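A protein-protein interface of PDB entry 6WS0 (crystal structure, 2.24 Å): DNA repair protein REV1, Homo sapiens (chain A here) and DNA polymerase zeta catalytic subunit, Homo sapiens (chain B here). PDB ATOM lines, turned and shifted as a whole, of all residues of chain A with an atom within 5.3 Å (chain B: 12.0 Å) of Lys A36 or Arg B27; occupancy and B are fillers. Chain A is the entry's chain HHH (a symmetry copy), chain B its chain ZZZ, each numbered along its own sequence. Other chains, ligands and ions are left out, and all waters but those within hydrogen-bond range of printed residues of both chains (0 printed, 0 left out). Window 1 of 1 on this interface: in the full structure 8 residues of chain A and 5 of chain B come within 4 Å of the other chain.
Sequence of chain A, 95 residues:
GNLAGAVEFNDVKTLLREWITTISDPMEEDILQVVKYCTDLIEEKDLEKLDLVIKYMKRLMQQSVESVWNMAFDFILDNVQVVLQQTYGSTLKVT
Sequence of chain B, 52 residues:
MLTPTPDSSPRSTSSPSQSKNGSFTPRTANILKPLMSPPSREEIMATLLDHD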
ATOM      1  N   ASN A   2      22.362 -11.292  22.179  1.00  0.00           N
ATOM      2  CA  ASN A   2      21.547 -11.552  20.957  1.00  0.00           C
ATOM      3  C   ASN A   2      22.288 -11.075  19.697  1.00  0.00           C
ATOM      4  O   ASN A   2      22.386 -11.880  18.754  1.00  0.00           O
ATOM      5  CB  ASN A   2      20.151 -10.919  21.049  1.00  0.00           C
ATOM      6  CG  ASN A   2      20.106  -9.438  20.716  1.00  0.00           C
ATOM      7  OD1 ASN A   2      21.030  -8.686  21.024  1.00  0.00           O
ATOM      8  ND2 ASN A   2      19.025  -9.000  20.084  1.00  0.00           N
ATOM      9  N   LEU A  32      22.769   1.484  18.205  1.00  0.00           N
ATOM     10  CA  LEU A  32      22.054   1.386  19.510  1.00  0.00           C
ATOM     11  C   LEU A  32      21.958  -0.087  19.907  1.00  0.00           C
ATOM     12  O   LEU A  32      22.131  -0.409  21.105  1.00  0.00           O
ATOM     13  CB  LEU A  32      20.682   2.055  19.405  1.00  0.00           C
ATOM     14  CG  LEU A  32      20.738   3.579  19.367  1.00  0.00           C
ATOM     15  CD1 LEU A  32      19.357   4.178  19.493  1.00  0.00           C
ATOM     16  CD2 LEU A  32      21.606   4.116  20.478  1.00  0.00           C
ATOM     17  N   GLN A  33      21.711  -0.938  18.912  1.00  0.00           N
ATOM     18  CA  GLN A  33      21.667  -2.407  19.051  1.00  0.00           C
ATOM     19  C   GLN A  33      23.030  -2.891  19.581  1.00  0.00           C
ATOM     20  O   GLN A  33      23.064  -3.856  20.336  1.00  0.00           O
ATOM     21  CB  GLN A  33      21.301  -3.011  17.693  1.00  0.00           C
ATOM     22  CG  GLN A  33      20.271  -4.129  17.764  1.00  0.00           C
ATOM     23  CD  GLN A  33      18.874  -3.590  17.921  1.00  0.00           C
ATOM     24  OE1 GLN A  33      18.445  -2.721  17.163  1.00  0.00           O
ATOM     25  NE2 GLN A  33      18.168  -4.083  18.927  1.00  0.00           N
ATOM     26  N   VAL A  34      24.153  -2.288  19.196  1.00  0.00           N
ATOM     27  CA  VAL A  34      25.452  -2.778  19.732  1.00  0.00           C
ATOM     28  C   VAL A  34      25.578  -2.266  21.159  1.00  0.00           C
ATOM     29  O   VAL A  34      26.070  -3.000  22.024  1.00  0.00           O
ATOM     30  CB  VAL A  34      26.641  -2.342  18.865  1.00  0.00           C
ATOM     31  CG1 VAL A  34      27.961  -2.517  19.596  1.00  0.00           C
ATOM     32  CG2 VAL A  34      26.619  -3.078  17.526  1.00  0.00           C
ATOM     33  N   VAL A  35      25.163  -1.034  21.426  1.00  0.00           N
ATOM     34  CA  VAL A  35      25.200  -0.593  22.840  1.00  0.00           C
ATOM     35  C   VAL A  35      24.378  -1.547  23.735  1.00  0.00           C
ATOM     36  O   VAL A  35      24.873  -1.893  24.793  1.00  0.00           O
ATOM     37  CB  VAL A  35      24.723   0.850  22.995  1.00  0.00           C
ATOM     38  CG1 VAL A  35      24.530   1.123  24.482  1.00  0.00           C
ATOM     39  CG2 VAL A  35      25.704   1.813  22.329  1.00  0.00           C
ATOM     40  N   LYS A  36      23.151  -1.901  23.361  1.00  0.00           N
ATOM     41  CA  LYS A  36      22.251  -2.790  24.150  1.00  0.00           C
ATOM     42  C   LYS A  36      22.868  -4.191  24.282  1.00  0.00           C
ATOM     43  O   LYS A  36      22.901  -4.758  25.421  1.00  0.00           O
ATOM     44  CB  LYS A  36      20.898  -2.885  23.452  1.00  0.00           C
ATOM     45  CG  LYS A  36      20.023  -4.060  23.867  1.00  0.00           C
ATOM     46  CD  LYS A  36      18.744  -3.703  24.575  1.00  0.00           C
ATOM     47  CE  LYS A  36      17.722  -4.823  24.501  1.00  0.00           C
ATOM     48  NZ  LYS A  36      18.194  -6.070  25.154  1.00  0.00           N
ATOM     49  N   TYR A  37      23.389  -4.734  23.180  1.00  0.00           N
ATOM     50  CA  TYR A  37      24.248  -5.936  23.220  1.00  0.00           C
ATOM     51  C   TYR A  37      25.315  -5.745  24.317  1.00  0.00           C
ATOM     52  O   TYR A  37      25.406  -6.540  25.238  1.00  0.00           O
ATOM     53  CB  TYR A  37      24.881  -6.266  21.865  1.00  0.00           C
ATOM     54  CG  TYR A  37      25.765  -7.488  21.937  1.00  0.00           C
ATOM     55  CD1 TYR A  37      25.216  -8.743  22.135  1.00  0.00           C
ATOM     56  CD2 TYR A  37      27.148  -7.391  21.854  1.00  0.00           C
ATOM     57  CE1 TYR A  37      26.012  -9.873  22.243  1.00  0.00           C
ATOM     58  CE2 TYR A  37      27.958  -8.513  21.930  1.00  0.00           C
ATOM     59  CZ  TYR A  37      27.384  -9.752  22.149  1.00  0.00           C
ATOM     60  OH  TYR A  37      28.166 -10.857  22.267  1.00  0.00           O
ATOM     61  N   CYS A  38      26.109  -4.688  24.283  1.00  0.00           N
ATOM     62  CA  CYS A  38      27.190  -4.525  25.303  1.00  0.00           C
ATOM     63  C   CYS A  38      26.620  -4.419  26.731  1.00  0.00           C
ATOM     64  O   CYS A  38      27.182  -5.022  27.650  1.00  0.00           O
ATOM     65  CB  CYS A  38      28.068  -3.335  24.973  1.00  0.00           C
ATOM     66  SG  CYS A  38      29.092  -3.639  23.517  1.00  0.00           S
ATOM     67  N   THR A  39      25.554  -3.668  26.963  1.00  0.00           N
ATOM     68  CA  THR A  39      25.014  -3.504  28.348  1.00  0.00           C
ATOM     69  C   THR A  39      24.396  -4.830  28.819  1.00  0.00           C
ATOM     70  O   THR A  39      24.458  -5.100  30.027  1.00  0.00           O
ATOM     71  CB  THR A  39      24.093  -2.285  28.427  1.00  0.00           C
ATOM     72  OG1 THR A  39      23.084  -2.381  27.441  1.00  0.00           O
ATOM     73  CG2 THR A  39      24.837  -0.997  28.151  1.00  0.00           C
ATOM     74  N   ASP A  40      23.848  -5.643  27.906  1.00  0.00           N
ATOM     75  CA  ASP A  40      23.300  -6.989  28.216  1.00  0.00           C
ATOM     76  C   ASP A  40      24.450  -7.889  28.671  1.00  0.00           C
ATOM     77  O   ASP A  40      24.281  -8.576  29.658  1.00  0.00           O
ATOM     78  CB  ASP A  40      22.581  -7.608  27.020  1.00  0.00           C
ATOM     79  CG  ASP A  40      21.230  -6.993  26.730  1.00  0.00           C
ATOM     80  OD1 ASP A  40      20.751  -6.225  27.600  1.00  0.00           O
ATOM     81  OD2 ASP A  40      20.668  -7.264  25.634  1.00  0.00           O
ATOM     82  N   LEU A  41      25.597  -7.867  27.989  1.00  0.00           N
ATOM     83  CA  LEU A  41      26.779  -8.595  28.478  1.00  0.00           C
ATOM     84  C   LEU A  41      27.050  -8.175  29.935  1.00  0.00           C
ATOM     85  O   LEU A  41      27.442  -9.005  30.754  1.00  0.00           O
ATOM     86  CB  LEU A  41      27.982  -8.237  27.612  1.00  0.00           C
ATOM     87  CG  LEU A  41      27.963  -8.724  26.173  1.00  0.00           C
ATOM     88  CD1 LEU A  41      29.246  -8.302  25.482  1.00  0.00           C
ATOM     89  CD2 LEU A  41      27.820 -10.228  26.113  1.00  0.00           C
ATOM     90  N   ARG B  27      14.349  -6.422  16.796  1.00  0.00           N
ATOM     91  CA  ARG B  27      14.196  -6.091  18.251  1.00  0.00           C
ATOM     92  C   ARG B  27      14.471  -4.595  18.468  1.00  0.00           C
ATOM     93  O   ARG B  27      15.484  -4.285  19.122  1.00  0.00           O
ATOM     94  CB  ARG B  27      15.143  -6.953  19.095  1.00  0.00           C
ATOM     95  CG  ARG B  27      14.716  -8.408  19.251  1.00  0.00           C
ATOM     96  CD  ARG B  27      15.499  -9.143  20.329  1.00  0.00           C
ATOM     97  NE  ARG B  27      15.519  -8.443  21.619  1.00  0.00           N
ATOM     98  CZ  ARG B  27      15.178  -8.958  22.805  1.00  0.00           C
ATOM     99  NH1 ARG B  27      14.776 -10.216  22.912  1.00  0.00           N
ATOM    100  NH2 ARG B  27      15.253  -8.200  23.892  1.00  0.00           N
ATOM    101  N   THR B  28      13.589  -3.716  17.964  1.00  0.00           N
ATOM    102  CA  THR B  28      13.794  -2.243  17.832  1.00  0.00           C
ATOM    103  C   THR B  28      14.124  -1.630  19.200  1.00  0.00           C
ATOM    104  O   THR B  28      13.557  -2.111  20.216  1.00  0.00           O
ATOM    105  CB  THR B  28      12.591  -1.551  17.175  1.00  0.00           C
ATOM    106  OG1 THR B  28      12.039  -2.422  16.189  1.00  0.00           O
ATOM    107  CG2 THR B  28      12.962  -0.233  16.530  1.00  0.00           C
ATOM    108  N   ALA B  29      14.978  -0.591  19.196  1.00  0.00           N
ATOM    109  CA  ALA B  29      15.813  -0.124  20.335  1.00  0.00           C
ATOM    110  C   ALA B  29      15.517   1.350  20.659  1.00  0.00           C
ATOM    111  O   ALA B  29      16.438   2.175  20.607  1.00  0.00           O
ATOM    112  CB  ALA B  29      17.271  -0.307  19.985  1.00  0.00           C
ATOM    113  N   ASN B  30      14.265   1.665  20.978  1.00  0.00           N
ATOM    114  CA  ASN B  30      13.752   3.051  21.114  1.00  0.00           C
ATOM    115  C   ASN B  30      13.189   3.225  22.534  1.00  0.00           C
ATOM    116  O   ASN B  30      12.425   4.207  22.807  1.00  0.00           O
ATOM    117  CB  ASN B  30      12.713   3.311  20.031  1.00  0.00           C
ATOM    118  CG  ASN B  30      11.501   2.457  20.290  1.00  0.00           C
ATOM    119  OD1 ASN B  30      11.614   1.231  20.304  1.00  0.00           O
ATOM    120  ND2 ASN B  30      10.378   3.101  20.581  1.00  0.00           N
ATOM    121  N   ILE B  31      13.585   2.345  23.446  1.00  0.00           N
ATOM    122  CA  ILE B  31      13.056   2.400  24.829  1.00  0.00           C
ATOM    123  C   ILE B  31      14.222   2.568  25.781  1.00  0.00           C
ATOM    124  O   ILE B  31      15.094   1.683  25.824  1.00  0.00           O
ATOM    125  CB  ILE B  31      12.161   1.201  25.158  1.00  0.00           C
ATOM    126  CG1 ILE B  31      11.069   1.042  24.094  1.00  0.00           C
ATOM    127  CG2 ILE B  31      11.584   1.368  26.564  1.00  0.00           C
ATOM    128  CD1 ILE B  31      10.329  -0.288  24.144  1.00  0.00           C
ATOM    129  N   LEU B  32      14.215   3.692  26.513  1.00  0.00           N
ATOM    130  CA  LEU B  32      15.327   4.053  27.430  1.00  0.00           C
ATOM    131  C   LEU B  32      14.807   3.995  28.870  1.00  0.00           C
ATOM    132  O   LEU B  32      13.645   4.361  29.090  1.00  0.00           O
ATOM    133  CB  LEU B  32      15.863   5.440  27.039  1.00  0.00           C
ATOM    134  CG  LEU B  32      16.698   5.500  25.751  1.00  0.00           C
ATOM    135  CD1 LEU B  32      16.954   6.930  25.316  1.00  0.00           C
ATOM    136  CD2 LEU B  32      18.037   4.799  25.958  1.00  0.00           C
ATOM    137  N   LYS B  33      15.632   3.553  29.809  1.00  0.00           N
ATOM    138  CA  LYS B  33      15.243   3.529  31.234  1.00  0.00           C
ATOM    139  C   LYS B  33      16.465   3.726  32.114  1.00  0.00           C
ATOM    140  O   LYS B  33      17.587   3.345  31.752  1.00  0.00           O
ATOM    141  CB  LYS B  33      14.581   2.199  31.580  1.00  0.00           C
ATOM    142  CG  LYS B  33      15.514   1.002  31.578  1.00  0.00           C
ATOM    143  CD  LYS B  33      14.808  -0.307  31.927  1.00  0.00           C
ATOM    144  CE  LYS B  33      14.273  -0.333  33.340  1.00  0.00           C
ATOM    145  NZ  LYS B  33      15.391  -0.552  34.274  1.00  0.00           N
ATOM    146  N   PRO B  34      16.265   4.312  33.313  1.00  0.00           N
ATOM    147  CA  PRO B  34      17.375   4.513  34.224  1.00  0.00           C
ATOM    148  C   PRO B  34      17.874   3.113  34.562  1.00  0.00           C
ATOM    149  O   PRO B  34      17.082   2.218  34.761  1.00  0.00           O
ATOM    150  CB  PRO B  34      16.770   5.267  35.419  1.00  0.00           C
ATOM    151  CG  PRO B  34      15.475   5.847  34.898  1.00  0.00           C
ATOM    152  CD  PRO B  34      14.997   4.862  33.836  1.00  0.00           C
ATOM    153  N   LEU B  35      19.183   2.950  34.626  1.00  0.00           N
ATOM    154  CA  LEU B  35      19.787   1.710  35.173  1.00  0.00           C
ATOM    155  C   LEU B  35      19.391   1.585  36.650  1.00  0.00           C
ATOM    156  O   LEU B  35      19.277   0.460  37.176  1.00  0.00           O
ATOM    157  CB  LEU B  35      21.304   1.819  35.043  1.00  0.00           C
ATOM    158  CG  LEU B  35      22.077   0.614  35.575  1.00  0.00           C
ATOM    159  CD1 LEU B  35      21.810  -0.633  34.723  1.00  0.00           C
ATOM    160  CD2 LEU B  35      23.559   0.916  35.623  1.00  0.00           C
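O of Arg B27 sits at hydrogen-bond distance from NE2 of Gln A33 (2.7 Å).
The backbone carbonyl oxygen (O) of Lys A36 sits at hydrogen-bond distance from the side-chain hydroxyl (OG1) of Thr A39, 3.1 Å away.
The side-chain carboxylate (OD2) of Asp A40 is in salt-bridge range of the side-chain amino group (NZ) of Lys A36, at 2.8 Å.
Of the 11 printed residues of chain A, 4 touch a printed residue of chain B.
Printed residues of chain A that touch a printed residue of chain B: Asn A2, Leu A32, Gln A33 and Lys A36.
Among the printed residues, no Asp or Glu carboxylate lies within 4 Å of a Lys or Arg side-chain nitrogen of the other chain.
Asn A2 touches just one residue of chain B: Arg B27 (3.5 Å).
Of the printed residues of chain B, Leu A32 touches Ala B29 (3.7 Å).
Of the printed residues of chain B, Gln A33 touches Arg B27 and Ala B29.
No residue of chain B comes within 4 Å of Val A34.
Val A35 touches none of the printed residues of chain B.
Of chain B, only Arg B27 (3.8 Å) comes within 4 Å of Lys A36.
No residue of chain B comes within 4 Å of Cys A38.
No residue of chain B comes within 4 Å of Thr A39.
No residue of chain B comes within 4 Å of Asp A40.
Arg B27 touches three residues of chain A.
Thr B28 touches none of the printed residues of chain A.
Of the printed residues of chain A, Ala B29 touches Leu A32 and Gln A33.
Asn B30 touches none of the printed residues of chain A.
The nearest printed residue of chain B that does not touch Leu A32 is Asn B30 (5.9 Å).
Among the printed residues, pairs that only touch across the chains: Asn A2 with Arg B27 (3.5 Å), Leu A32 with Ala B29 (3.7 Å), Lys A36 with Arg B27 (3.8 Å) and Gln A33 with Ala B29 (3.9 Å).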
